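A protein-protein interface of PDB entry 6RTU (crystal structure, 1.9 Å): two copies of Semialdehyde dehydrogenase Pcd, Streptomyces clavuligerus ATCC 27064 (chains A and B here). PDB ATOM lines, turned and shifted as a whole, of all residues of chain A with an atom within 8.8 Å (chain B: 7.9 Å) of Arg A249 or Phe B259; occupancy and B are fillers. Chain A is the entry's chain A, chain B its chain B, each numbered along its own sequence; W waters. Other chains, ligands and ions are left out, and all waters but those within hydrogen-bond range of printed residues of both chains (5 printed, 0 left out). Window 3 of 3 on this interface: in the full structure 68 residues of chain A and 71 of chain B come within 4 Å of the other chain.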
ATOM      1  N   ALA A 241       4.571 -23.658   3.484  1.00  0.00           N
ATOM      2  CA  ALA A 241       5.739 -24.339   2.922  1.00  0.00           C
ATOM      3  C   ALA A 241       7.008 -23.746   3.513  1.00  0.00           C
ATOM      4  O   ALA A 241       7.281 -22.552   3.342  1.00  0.00           O
ATOM      5  CB  ALA A 241       5.761 -24.249   1.390  1.00  0.00           C
ATOM      6  N   GLY A 243      11.257 -24.426   4.083  1.00  0.00           N
ATOM      7  CA  GLY A 243      12.415 -25.177   3.644  1.00  0.00           C
ATOM      8  C   GLY A 243      13.027 -24.667   2.357  1.00  0.00           C
ATOM      9  O   GLY A 243      12.384 -23.937   1.590  1.00  0.00           O
ATOM     10  N   SER A 244      14.284 -25.041   2.123  1.00  0.00           N
ATOM     11  CA  SER A 244      15.010 -24.640   0.921  1.00  0.00           C
ATOM     12  C   SER A 244      14.950 -25.746  -0.136  1.00  0.00           C
ATOM     13  O   SER A 244      14.078 -25.731  -1.013  1.00  0.00           O
ATOM     14  CB  SER A 244      16.466 -24.295   1.269  1.00  0.00           C
ATOM     15  OG  SER A 244      17.035 -23.405   0.323  1.00  0.00           O
ATOM     16  N   GLY A 248       9.441 -25.306  -3.805  1.00  0.00           N
ATOM     17  CA  GLY A 248       8.928 -24.365  -2.824  1.00  0.00           C
ATOM     18  C   GLY A 248       8.693 -22.988  -3.422  1.00  0.00           C
ATOM     19  O   GLY A 248       7.694 -22.318  -3.135  1.00  0.00           O
ATOM     20  N   ARG A 249       9.619 -22.557  -4.280  1.00  0.00           N
ATOM     21  CA  ARG A 249       9.515 -21.221  -4.852  1.00  0.00           C
ATOM     22  C   ARG A 249       8.366 -21.096  -5.849  1.00  0.00           C
ATOM     23  O   ARG A 249       7.975 -19.971  -6.182  1.00  0.00           O
ATOM     24  CB  ARG A 249      10.849 -20.842  -5.500  1.00  0.00           C
ATOM     25  CG  ARG A 249      11.919 -20.431  -4.484  1.00  0.00           C
ATOM     26  CD  ARG A 249      13.263 -20.070  -5.150  1.00  0.00           C
ATOM     27  NE  ARG A 249      13.274 -18.693  -5.644  1.00  0.00           N
ATOM     28  CZ  ARG A 249      14.370 -18.024  -5.999  1.00  0.00           C
ATOM     29  NH1 ARG A 249      15.563 -18.598  -5.899  1.00  0.00           N
ATOM     30  NH2 ARG A 249      14.270 -16.777  -6.446  1.00  0.00           N
ATOM     31  N   ALA A 250       7.816 -22.209  -6.327  1.00  0.00           N
ATOM     32  CA  ALA A 250       6.651 -22.166  -7.200  1.00  0.00           C
ATOM     33  C   ALA A 250       5.333 -22.195  -6.436  1.00  0.00           C
ATOM     34  O   ALA A 250       4.285 -21.966  -7.042  1.00  0.00           O
ATOM     35  CB  ALA A 250       6.690 -23.334  -8.192  1.00  0.00           C
ATOM     36  N   VAL A 251       5.363 -22.456  -5.125  1.00  0.00           N
ATOM     37  CA  VAL A 251       4.125 -22.605  -4.363  1.00  0.00           C
ATOM     38  C   VAL A 251       3.333 -21.300  -4.351  1.00  0.00           C
ATOM     39  O   VAL A 251       2.108 -21.299  -4.526  1.00  0.00           O
ATOM     40  CB  VAL A 251       4.432 -23.095  -2.935  1.00  0.00           C
ATOM     41  CG1 VAL A 251       3.187 -23.024  -2.068  1.00  0.00           C
ATOM     42  CG2 VAL A 251       4.970 -24.528  -2.973  1.00  0.00           C
ATOM     43  N   GLY A 252       4.015 -20.174  -4.158  1.00  0.00           N
ATOM     44  CA  GLY A 252       3.358 -18.890  -4.035  1.00  0.00           C
ATOM     45  C   GLY A 252       2.449 -18.535  -5.202  1.00  0.00           C
ATOM     46  O   GLY A 252       1.244 -18.309  -5.034  1.00  0.00           O
ATOM     47  N   PRO A 253       3.015 -18.477  -6.411  1.00  0.00           N
ATOM     48  CA  PRO A 253       2.190 -18.129  -7.584  1.00  0.00           C
ATOM     49  C   PRO A 253       1.068 -19.114  -7.856  1.00  0.00           C
ATOM     50  O   PRO A 253      -0.027 -18.707  -8.253  1.00  0.00           O
ATOM     51  CB  PRO A 253       3.203 -18.114  -8.738  1.00  0.00           C
ATOM     52  CG  PRO A 253       4.539 -17.962  -8.091  1.00  0.00           C
ATOM     53  CD  PRO A 253       4.450 -18.576  -6.737  1.00  0.00           C
ATOM     54  N   ARG A 254       1.307 -20.409  -7.654  1.00  0.00           N
ATOM     55  CA  ARG A 254       0.288 -21.397  -8.000  1.00  0.00           C
ATOM     56  C   ARG A 254      -0.899 -21.326  -7.047  1.00  0.00           C
ATOM     57  O   ARG A 254      -2.051 -21.453  -7.468  1.00  0.00           O
ATOM     58  CB  ARG A 254       0.900 -22.795  -8.008  1.00  0.00           C
ATOM     59  CG  ARG A 254       2.073 -22.882  -8.973  1.00  0.00           C
ATOM     60  CD  ARG A 254       2.082 -24.192  -9.712  1.00  0.00           C
ATOM     61  NE  ARG A 254       2.356 -25.311  -8.825  1.00  0.00           N
ATOM     62  CZ  ARG A 254       1.629 -26.420  -8.813  1.00  0.00           C
ATOM     63  NH1 ARG A 254       0.566 -26.517  -9.604  1.00  0.00           N
ATOM     64  NH2 ARG A 254       1.962 -27.413  -8.002  1.00  0.00           N
ATOM     65  N   VAL A 255      -0.643 -21.111  -5.761  1.00  0.00           N
ATOM     66  CA  VAL A 255      -1.742 -20.934  -4.821  1.00  0.00           C
ATOM     67  C   VAL A 255      -2.417 -19.587  -5.049  1.00  0.00           C
ATOM     68  O   VAL A 255      -3.648 -19.483  -5.003  1.00  0.00           O
ATOM     69  CB  VAL A 255      -1.232 -21.095  -3.377  1.00  0.00           C
ATOM     70  CG1 VAL A 255      -2.330 -20.778  -2.366  1.00  0.00           C
ATOM     71  CG2 VAL A 255      -0.708 -22.513  -3.168  1.00  0.00           C
ATOM     72  N   LEU A 264       5.119 -18.767   3.468  1.00  0.00           N
ATOM     73  CA  LEU A 264       6.329 -19.202   2.778  1.00  0.00           C
ATOM     74  C   LEU A 264       7.571 -18.791   3.560  1.00  0.00           C
ATOM     75  O   LEU A 264       7.723 -17.619   3.921  1.00  0.00           O
ATOM     76  CB  LEU A 264       6.401 -18.599   1.374  1.00  0.00           C
ATOM     77  CG  LEU A 264       5.247 -18.876   0.417  1.00  0.00           C
ATOM     78  CD1 LEU A 264       5.361 -17.961  -0.833  1.00  0.00           C
ATOM     79  CD2 LEU A 264       5.230 -20.343   0.031  1.00  0.00           C
ATOM     80  N   GLU A 265       8.459 -19.754   3.803  1.00  0.00           N
ATOM     81  CA  GLU A 265       9.783 -19.498   4.373  1.00  0.00           C
ATOM     82  C   GLU A 265      10.740 -20.386   3.581  1.00  0.00           C
ATOM     83  O   GLU A 265      10.839 -21.591   3.837  1.00  0.00           O
ATOM     84  CB  GLU A 265       9.824 -19.786   5.870  1.00  0.00           C
ATOM     85  CG  GLU A 265      11.110 -19.294   6.573  1.00  0.00           C
ATOM     86  CD  GLU A 265      12.311 -20.118   6.180  1.00  0.00           C
ATOM     87  OE1 GLU A 265      12.469 -21.226   6.743  1.00  0.00           O
ATOM     88  OE2 GLU A 265      13.075 -19.676   5.286  1.00  0.00           O
ATOM     89  N   LEU A 266      11.444 -19.779   2.629  1.00  0.00           N
ATOM     90  CA  LEU A 266      12.027 -20.496   1.501  1.00  0.00           C
ATOM     91  C   LEU A 266      13.547 -20.578   1.523  1.00  0.00           C
ATOM     92  O   LEU A 266      14.141 -21.098   0.569  1.00  0.00           O
ATOM     93  CB  LEU A 266      11.587 -19.838   0.190  1.00  0.00           C
ATOM     94  CG  LEU A 266      10.081 -19.727  -0.052  1.00  0.00           C
ATOM     95  CD1 LEU A 266       9.835 -19.057  -1.399  1.00  0.00           C
ATOM     96  CD2 LEU A 266       9.411 -21.093  -0.007  1.00  0.00           C
ATOM     97  N   GLY A 267      14.195 -20.089   2.571  1.00  0.00           N
ATOM     98  CA  GLY A 267      15.641 -20.169   2.634  1.00  0.00           C
ATOM     99  C   GLY A 267      16.231 -18.875   3.150  1.00  0.00           C
ATOM    100  O   GLY A 267      15.522 -17.879   3.292  1.00  0.00           O
ATOM    101  N   GLU A 398      24.849 -16.472  -3.216  1.00  0.00           N
ATOM    102  CA  GLU A 398      24.040 -17.679  -3.359  1.00  0.00           C
ATOM    103  C   GLU A 398      24.041 -18.482  -2.066  1.00  0.00           C
ATOM    104  O   GLU A 398      25.069 -18.617  -1.398  1.00  0.00           O
ATOM    105  CB  GLU A 398      24.551 -18.546  -4.512  1.00  0.00           C
ATOM    106  CG  GLU A 398      24.202 -17.969  -5.874  1.00  0.00           C
ATOM    107  CD  GLU A 398      25.047 -18.545  -7.007  1.00  0.00           C
ATOM    108  OE1 GLU A 398      25.364 -17.792  -7.966  1.00  0.00           O
ATOM    109  OE2 GLU A 398      25.394 -19.747  -6.933  1.00  0.00           O
ATOM    110  N   GLU A 399      22.873 -18.988  -1.699  1.00  0.00           N
ATOM    111  CA  GLU A 399      22.750 -19.874  -0.548  1.00  0.00           C
ATOM    112  C   GLU A 399      23.157 -21.279  -0.979  1.00  0.00           C
ATOM    113  O   GLU A 399      22.521 -21.861  -1.863  1.00  0.00           O
ATOM    114  CB  GLU A 399      21.309 -19.849  -0.028  1.00  0.00           C
ATOM    115  CG  GLU A 399      20.937 -20.963   0.956  1.00  0.00           C
ATOM    116  CD  GLU A 399      19.418 -21.140   1.076  1.00  0.00           C
ATOM    117  OE1 GLU A 399      18.922 -21.490   2.167  1.00  0.00           O
ATOM    118  OE2 GLU A 399      18.715 -20.923   0.068  1.00  0.00           O
ATOM    119  N   PRO A 424      19.715 -11.568  -2.041  1.00  0.00           N
ATOM    120  CA  PRO A 424      18.274 -11.687  -2.326  1.00  0.00           C
ATOM    121  C   PRO A 424      17.448 -12.244  -1.178  1.00  0.00           C
ATOM    122  O   PRO A 424      16.229 -12.036  -1.178  1.00  0.00           O
ATOM    123  CB  PRO A 424      18.227 -12.632  -3.540  1.00  0.00           C
ATOM    124  CG  PRO A 424      19.547 -13.314  -3.567  1.00  0.00           C
ATOM    125  CD  PRO A 424      20.533 -12.350  -2.987  1.00  0.00           C
ATOM    126  N   GLN A 425      18.047 -12.960  -0.229  1.00  0.00           N
ATOM    127  CA  GLN A 425      17.307 -13.542   0.883  1.00  0.00           C
ATOM    128  C   GLN A 425      17.164 -12.515   2.018  1.00  0.00           C
ATOM    129  O   GLN A 425      17.766 -11.440   1.995  1.00  0.00           O
ATOM    130  CB  GLN A 425      18.000 -14.822   1.376  1.00  0.00           C
ATOM    131  CG  GLN A 425      18.309 -15.874   0.268  1.00  0.00           C
ATOM    132  CD  GLN A 425      19.615 -15.580  -0.487  1.00  0.00           C
ATOM    133  OE1 GLN A 425      20.282 -14.570  -0.236  1.00  0.00           O
ATOM    134  NE2 GLN A 425      19.969 -16.455  -1.421  1.00  0.00           N
ATOM    135  N   GLY A 470      10.811 -14.567   7.286  1.00  0.00           N
ATOM    136  CA  GLY A 470      11.702 -13.586   6.696  1.00  0.00           C
ATOM    137  C   GLY A 470      11.111 -12.848   5.506  1.00  0.00           C
ATOM    138  O   GLY A 470       9.963 -13.064   5.113  1.00  0.00           O
ATOM    139  N   GLU A 471      11.946 -11.987   4.916  1.00  0.00           N
ATOM    140  CA  GLU A 471      11.553 -11.003   3.913  1.00  0.00           C
ATOM    141  C   GLU A 471      12.249 -11.305   2.581  1.00  0.00           C
ATOM    142  O   GLU A 471      13.005 -12.267   2.461  1.00  0.00           O
ATOM    143  CB  GLU A 471      11.884  -9.590   4.415  1.00  0.00           C
ATOM    144  CG  GLU A 471      11.052  -9.180   5.633  1.00  0.00           C
ATOM    145  CD  GLU A 471       9.550  -9.240   5.342  1.00  0.00           C
ATOM    146  OE1 GLU A 471       9.113  -8.684   4.304  1.00  0.00           O
ATOM    147  OE2 GLU A 471       8.811  -9.869   6.134  1.00  0.00           O
ATOM    148  N   LYS A 472      11.965 -10.481   1.568  1.00  0.00           N
ATOM    149  CA  LYS A 472      12.597 -10.571   0.228  1.00  0.00           C
ATOM    150  C   LYS A 472      12.331 -11.973  -0.321  1.00  0.00           C
ATOM    151  O   LYS A 472      11.179 -12.431  -0.241  1.00  0.00           O
ATOM    152  CB  LYS A 472      14.066 -10.153   0.348  1.00  0.00           C
ATOM    153  CG  LYS A 472      14.231  -8.710   0.856  1.00  0.00           C
ATOM    154  CD  LYS A 472      15.520  -8.513   1.637  1.00  0.00           C
ATOM    155  CE  LYS A 472      16.736  -8.758   0.769  1.00  0.00           C
ATOM    156  NZ  LYS A 472      17.986  -8.810   1.600  1.00  0.00           N
ATOM    157  N   GLU A 473      13.332 -12.685  -0.864  1.00  0.00           N
ATOM    158  CA  GLU A 473      13.075 -13.991  -1.472  1.00  0.00           C
ATOM    159  C   GLU A 473      12.902 -15.108  -0.449  1.00  0.00           C
ATOM    160  O   GLU A 473      12.618 -16.244  -0.847  1.00  0.00           O
ATOM    161  CB  GLU A 473      14.187 -14.365  -2.475  1.00  0.00           C
ATOM    162  CG  GLU A 473      14.319 -13.372  -3.623  1.00  0.00           C
ATOM    163  CD  GLU A 473      15.060 -13.913  -4.848  1.00  0.00           C
ATOM    164  OE1 GLU A 473      15.661 -15.008  -4.783  1.00  0.00           O
ATOM    165  OE2 GLU A 473      15.048 -13.213  -5.884  1.00  0.00           O
ATOM    166  N   THR A 474      13.045 -14.818   0.849  1.00  0.00           N
ATOM    167  CA  THR A 474      12.639 -15.779   1.869  1.00  0.00           C
ATOM    168  C   THR A 474      11.132 -16.051   1.819  1.00  0.00           C
ATOM    169  O   THR A 474      10.689 -17.160   2.150  1.00  0.00           O
ATOM    170  CB  THR A 474      13.083 -15.283   3.252  1.00  0.00           C
ATOM    171  OG1 THR A 474      14.520 -15.253   3.297  1.00  0.00           O
ATOM    172  CG2 THR A 474      12.558 -16.191   4.373  1.00  0.00           C
ATOM    173  N   GLY A 475      10.327 -15.083   1.380  1.00  0.00           N
ATOM    174  CA  GLY A 475       8.941 -15.347   1.026  1.00  0.00           C
ATOM    175  C   GLY A 475       7.897 -14.622   1.851  1.00  0.00           C
ATOM    176  O   GLY A 475       6.724 -14.613   1.461  1.00  0.00           O
ATOM    177  N   GLY A 476       8.253 -14.032   2.987  1.00  0.00           N
ATOM    178  CA  GLY A 476       7.336 -13.144   3.683  1.00  0.00           C
ATOM    179  C   GLY A 476       6.429 -13.770   4.728  1.00  0.00           C
ATOM    180  O   GLY A 476       5.781 -13.023   5.477  1.00  0.00           O
ATOM    181  N   GLY A 477       6.343 -15.098   4.812  1.00  0.00           N
ATOM    182  CA  GLY A 477       5.436 -15.708   5.769  1.00  0.00           C
ATOM    183  C   GLY A 477       5.935 -15.592   7.200  1.00  0.00           C
ATOM    184  O   GLY A 477       7.122 -15.374   7.451  1.00  0.00           O
ATOM    185  N   VAL B 236       8.796  -2.535  -6.231  1.00  0.00           N
ATOM    186  CA  VAL B 236       7.482  -2.270  -5.649  1.00  0.00           C
ATOM    187  C   VAL B 236       7.082  -3.460  -4.779  1.00  0.00           C
ATOM    188  O   VAL B 236       6.492  -4.428  -5.277  1.00  0.00           O
ATOM    189  CB  VAL B 236       6.450  -1.971  -6.751  1.00  0.00           C
ATOM    190  CG1 VAL B 236       5.055  -1.808  -6.166  1.00  0.00           C
ATOM    191  CG2 VAL B 236       6.867  -0.707  -7.535  1.00  0.00           C
ATOM    192  N   PRO B 237       7.397  -3.442  -3.480  1.00  0.00           N
ATOM    193  CA  PRO B 237       7.158  -4.633  -2.648  1.00  0.00           C
ATOM    194  C   PRO B 237       5.701  -4.888  -2.313  1.00  0.00           C
ATOM    195  O   PRO B 237       5.382  -6.004  -1.893  1.00  0.00           O
ATOM    196  CB  PRO B 237       7.972  -4.343  -1.376  1.00  0.00           C
ATOM    197  CG  PRO B 237       8.099  -2.831  -1.351  1.00  0.00           C
ATOM    198  CD  PRO B 237       8.233  -2.445  -2.797  1.00  0.00           C
ATOM    199  N   LEU B 238       4.815  -3.904  -2.461  1.00  0.00           N
ATOM    200  CA  LEU B 238       3.393  -4.081  -2.201  1.00  0.00           C
ATOM    201  C   LEU B 238       2.587  -3.494  -3.357  1.00  0.00           C
ATOM    202  O   LEU B 238       2.803  -2.339  -3.745  1.00  0.00           O
ATOM    203  CB  LEU B 238       2.987  -3.406  -0.871  1.00  0.00           C
ATOM    204  CG  LEU B 238       1.479  -3.302  -0.613  1.00  0.00           C
ATOM    205  CD1 LEU B 238       0.806  -4.699  -0.562  1.00  0.00           C
ATOM    206  CD2 LEU B 238       1.171  -2.498   0.663  1.00  0.00           C
ATOM    207  N   PRO B 253      -0.921 -13.701  -8.802  1.00  0.00           N
ATOM    208  CA  PRO B 253       0.204 -14.603  -9.107  1.00  0.00           C
ATOM    209  C   PRO B 253       1.402 -13.892  -9.719  1.00  0.00           C
ATOM    210  O   PRO B 253       2.544 -14.291  -9.450  1.00  0.00           O
ATOM    211  CB  PRO B 253      -0.411 -15.643 -10.067  1.00  0.00           C
ATOM    212  CG  PRO B 253      -1.686 -15.064 -10.536  1.00  0.00           C
ATOM    213  CD  PRO B 253      -2.160 -14.082  -9.505  1.00  0.00           C
ATOM    214  N   ARG B 254       1.189 -12.840 -10.509  1.00  0.00           N
ATOM    215  CA  ARG B 254       2.317 -12.087 -11.057  1.00  0.00           C
ATOM    216  C   ARG B 254       3.198 -11.524  -9.953  1.00  0.00           C
ATOM    217  O   ARG B 254       4.429 -11.659  -9.992  1.00  0.00           O
ATOM    218  CB  ARG B 254       1.810 -10.950 -11.946  1.00  0.00           C
ATOM    219  CG  ARG B 254       1.404 -11.409 -13.326  1.00  0.00           C
ATOM    220  CD  ARG B 254       0.875 -10.255 -14.160  1.00  0.00           C
ATOM    221  NE  ARG B 254       1.946  -9.501 -14.811  1.00  0.00           N
ATOM    222  CZ  ARG B 254       1.768  -8.760 -15.901  1.00  0.00           C
ATOM    223  NH1 ARG B 254       0.566  -8.684 -16.461  1.00  0.00           N
ATOM    224  NH2 ARG B 254       2.790  -8.101 -16.438  1.00  0.00           N
ATOM    225  N   VAL B 255       2.587 -10.878  -8.956  1.00  0.00           N
ATOM    226  CA  VAL B 255       3.381 -10.277  -7.890  1.00  0.00           C
ATOM    227  C   VAL B 255       3.982 -11.359  -7.000  1.00  0.00           C
ATOM    228  O   VAL B 255       5.129 -11.247  -6.544  1.00  0.00           O
ATOM    229  CB  VAL B 255       2.529  -9.271  -7.096  1.00  0.00           C
ATOM    230  CG1 VAL B 255       3.298  -8.756  -5.885  1.00  0.00           C
ATOM    231  CG2 VAL B 255       2.128  -8.092  -7.986  1.00  0.00           C
ATOM    232  N   ALA B 256       3.221 -12.427  -6.740  1.00  0.00           N
ATOM    233  CA  ALA B 256       3.755 -13.533  -5.953  1.00  0.00           C
ATOM    234  C   ALA B 256       4.967 -14.164  -6.630  1.00  0.00           C
ATOM    235  O   ALA B 256       5.870 -14.661  -5.945  1.00  0.00           O
ATOM    236  CB  ALA B 256       2.669 -14.586  -5.720  1.00  0.00           C
ATOM    237  N   ALA B 257       5.008 -14.144  -7.971  1.00  0.00           N
ATOM    238  CA  ALA B 257       6.107 -14.772  -8.700  1.00  0.00           C
ATOM    239  C   ALA B 257       7.420 -14.045  -8.463  1.00  0.00           C
ATOM    240  O   ALA B 257       8.485 -14.657  -8.552  1.00  0.00           O
ATOM    241  CB  ALA B 257       5.789 -14.822 -10.197  1.00  0.00           C
ATOM    242  N   ARG B 258       7.371 -12.747  -8.151  1.00  0.00           N
ATOM    243  CA  ARG B 258       8.576 -11.996  -7.822  1.00  0.00           C
ATOM    244  C   ARG B 258       8.720 -11.755  -6.322  1.00  0.00           C
ATOM    245  O   ARG B 258       9.474 -10.863  -5.916  1.00  0.00           O
ATOM    246  CB  ARG B 258       8.607 -10.668  -8.577  1.00  0.00           C
ATOM    247  CG  ARG B 258       7.447  -9.712  -8.298  1.00  0.00           C
ATOM    248  CD  ARG B 258       7.678  -8.411  -9.079  1.00  0.00           C
ATOM    249  NE  ARG B 258       6.659  -7.394  -8.840  1.00  0.00           N
ATOM    250  CZ  ARG B 258       6.561  -6.687  -7.715  1.00  0.00           C
ATOM    251  NH1 ARG B 258       7.424  -6.893  -6.713  1.00  0.00           N
ATOM    252  NH2 ARG B 258       5.600  -5.773  -7.590  1.00  0.00           N
ATOM    253  N   PHE B 259       8.000 -12.527  -5.506  1.00  0.00           N
ATOM    254  CA  PHE B 259       8.057 -12.472  -4.042  1.00  0.00           C
ATOM    255  C   PHE B 259       7.559 -11.140  -3.483  1.00  0.00           C
ATOM    256  O   PHE B 259       7.958 -10.732  -2.389  1.00  0.00           O
ATOM    257  CB  PHE B 259       9.463 -12.766  -3.513  1.00  0.00           C
ATOM    258  CG  PHE B 259      10.015 -14.083  -3.965  1.00  0.00           C
ATOM    259  CD1 PHE B 259       9.504 -15.271  -3.467  1.00  0.00           C
ATOM    260  CD2 PHE B 259      11.043 -14.132  -4.896  1.00  0.00           C
ATOM    261  CE1 PHE B 259      10.007 -16.493  -3.891  1.00  0.00           C
ATOM    262  CE2 PHE B 259      11.560 -15.346  -5.321  1.00  0.00           C
ATOM    263  CZ  PHE B 259      11.039 -16.531  -4.817  1.00  0.00           C
ATOM    264  N   GLY B 260       6.670 -10.456  -4.207  1.00  0.00           N
ATOM    265  CA  GLY B 260       6.038  -9.269  -3.671  1.00  0.00           C
ATOM    266  C   GLY B 260       4.787  -9.601  -2.859  1.00  0.00           C
ATOM    267  O   GLY B 260       4.342 -10.746  -2.788  1.00  0.00           O
ATOM    268  N   ARG B 261       4.217  -8.567  -2.257  1.00  0.00           N
ATOM    269  CA  ARG B 261       2.991  -8.671  -1.477  1.00  0.00           C
ATOM    270  C   ARG B 261       1.837  -8.024  -2.246  1.00  0.00           C
ATOM    271  O   ARG B 261       2.033  -7.055  -2.986  1.00  0.00           O
ATOM    272  CB  ARG B 261       3.193  -7.986  -0.108  1.00  0.00           C
ATOM    273  CG  ARG B 261       2.146  -8.280   0.970  1.00  0.00           C
ATOM    274  CD  ARG B 261       2.419  -7.422   2.235  1.00  0.00           C
ATOM    275  NE  ARG B 261       3.626  -7.827   2.963  1.00  0.00           N
ATOM    276  CZ  ARG B 261       4.177  -7.126   3.957  1.00  0.00           C
ATOM    277  NH1 ARG B 261       3.645  -5.970   4.326  1.00  0.00           N
ATOM    278  NH2 ARG B 261       5.270  -7.572   4.579  1.00  0.00           N
ATOM    279  N   THR B 262       0.620  -8.547  -2.068  1.00  0.00           N
ATOM    280  CA  THR B 262      -0.559  -7.900  -2.637  1.00  0.00           C
ATOM    281  C   THR B 262      -1.653  -7.702  -1.598  1.00  0.00           C
ATOM    282  O   THR B 262      -1.784  -8.475  -0.642  1.00  0.00           O
ATOM    283  CB  THR B 262      -1.182  -8.675  -3.805  1.00  0.00           C
ATOM    284  OG1 THR B 262      -1.578  -9.981  -3.363  1.00  0.00           O
ATOM    285  CG2 THR B 262      -0.196  -8.798  -4.963  1.00  0.00           C
HETATM  286  O   HOH W   1       3.202 -10.865   4.540  1.00  0.00           O
HETATM  287  O   HOH W   2       6.168 -13.303  -1.116  1.00  0.00           O
HETATM  288  O   HOH W   3       8.751 -11.597   0.335  1.00  0.00           O
HETATM  289  O   HOH W   4       8.587 -17.562  -7.723  1.00  0.00           O
HETATM  290  O   HOH W   5       6.139 -10.307   5.912  1.00  0.00           O
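Water W3 bridges O of Lys A472 (2.6 Å) and O of Phe B259 (3.0 Å). Water W5 lies within hydrogen-bond range of the side-chain carboxylate of Glu A471 (2.7 Å), the backbone carbonyl oxygen of Gly A476 (2.8 Å) and the guanidinium group of Arg B261 (3.2 Å). Water W4 lies within hydrogen-bond range of O of Arg A249 (2.9 Å) and O of Ala B257 (3.0 Å). Water W2 bridges O of Gly A475 (2.9 Å) and O of Phe B259 (3.4 Å). Water W1 bridges the guanidinium group of Arg B261 and the backbone carbonyl oxygen of Gly A476.
Hydrophobic or aromatic side chains of chain B within 4 Å of the printed part of chain A: Pro B253, Ala B256, Ala B257 and Phe B259. Of the 27 printed residues of chain A, 6 touch a printed residue of chain B. Hydrophobic or aromatic side chains of chain A within 4 Å of the printed part of chain B: Pro A253 and Leu A266.
CZ of Phe B259 touches NE of Arg A249, at 3.2 Å. Ala B256 touches Gly A252. Pro A253 touches Pro B253 (O to CB, 3.6 Å). CB of Ala B256 touches N of Pro A253 (3.97 Å). Ala B257 touches Pro A253 (CA to CG, 3.6 Å). Leu A266 touches Phe B259 (CD1 to CE1, 3.6 Å). O of Lys A472 touches CB of Phe B259 (3.7 Å). Phe B259 touches Glu A473 (CD2 to CG, 3.6 Å).
The guanidinium group of Arg A249 lies within salt-bridge range of the side-chain carboxylate of Glu A473, at 2.8 Å. The backbone NH (N) of Leu A266 lies within hydrogen-bond range of the backbone carbonyl oxygen (O) of Thr A474, 2.8 Å away. The backbone carbonyl oxygen (O) of Pro A424 is in hydrogen-bond range of the backbone NH (N) of Glu A473 (3.0 Å). O of Gln A425 is in hydrogen-bond range of NZ of Lys A472, 2.7 Å away.
Arg A249 touches just one residue of chain B: Phe B259. Of the printed residues of chain B, Gly A252 touches Ala B256. Printed residues of chain B within 4 Å of Pro A253: Pro B253 (3.6 Å), Ala B256 (3.97 Å) and Ala B257 (3.6 Å). Leu A264 touches none of the printed residues of chain B. Of the printed residues of chain B, Lys A472 touches Phe B259. Of the printed residues of chain B, Glu A473 touches Phe B259. Printed residues of chain A within 4 Å of Ala B256: Gly A252 (3.99 Å) and Pro A253 (3.97 Å). No residue of chain A comes within 4 Å of Gly B260. The nearest residue of chain B that does not touch Arg A249 is Ala B256 (5.7 Å). The nearest residue of chain A that does not touch Phe B259 is Gly A475 (4.5 Å).
Pro A253 touches its own counterpart, Pro B253. Positions printed for both chains: 253, 254 and 255.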
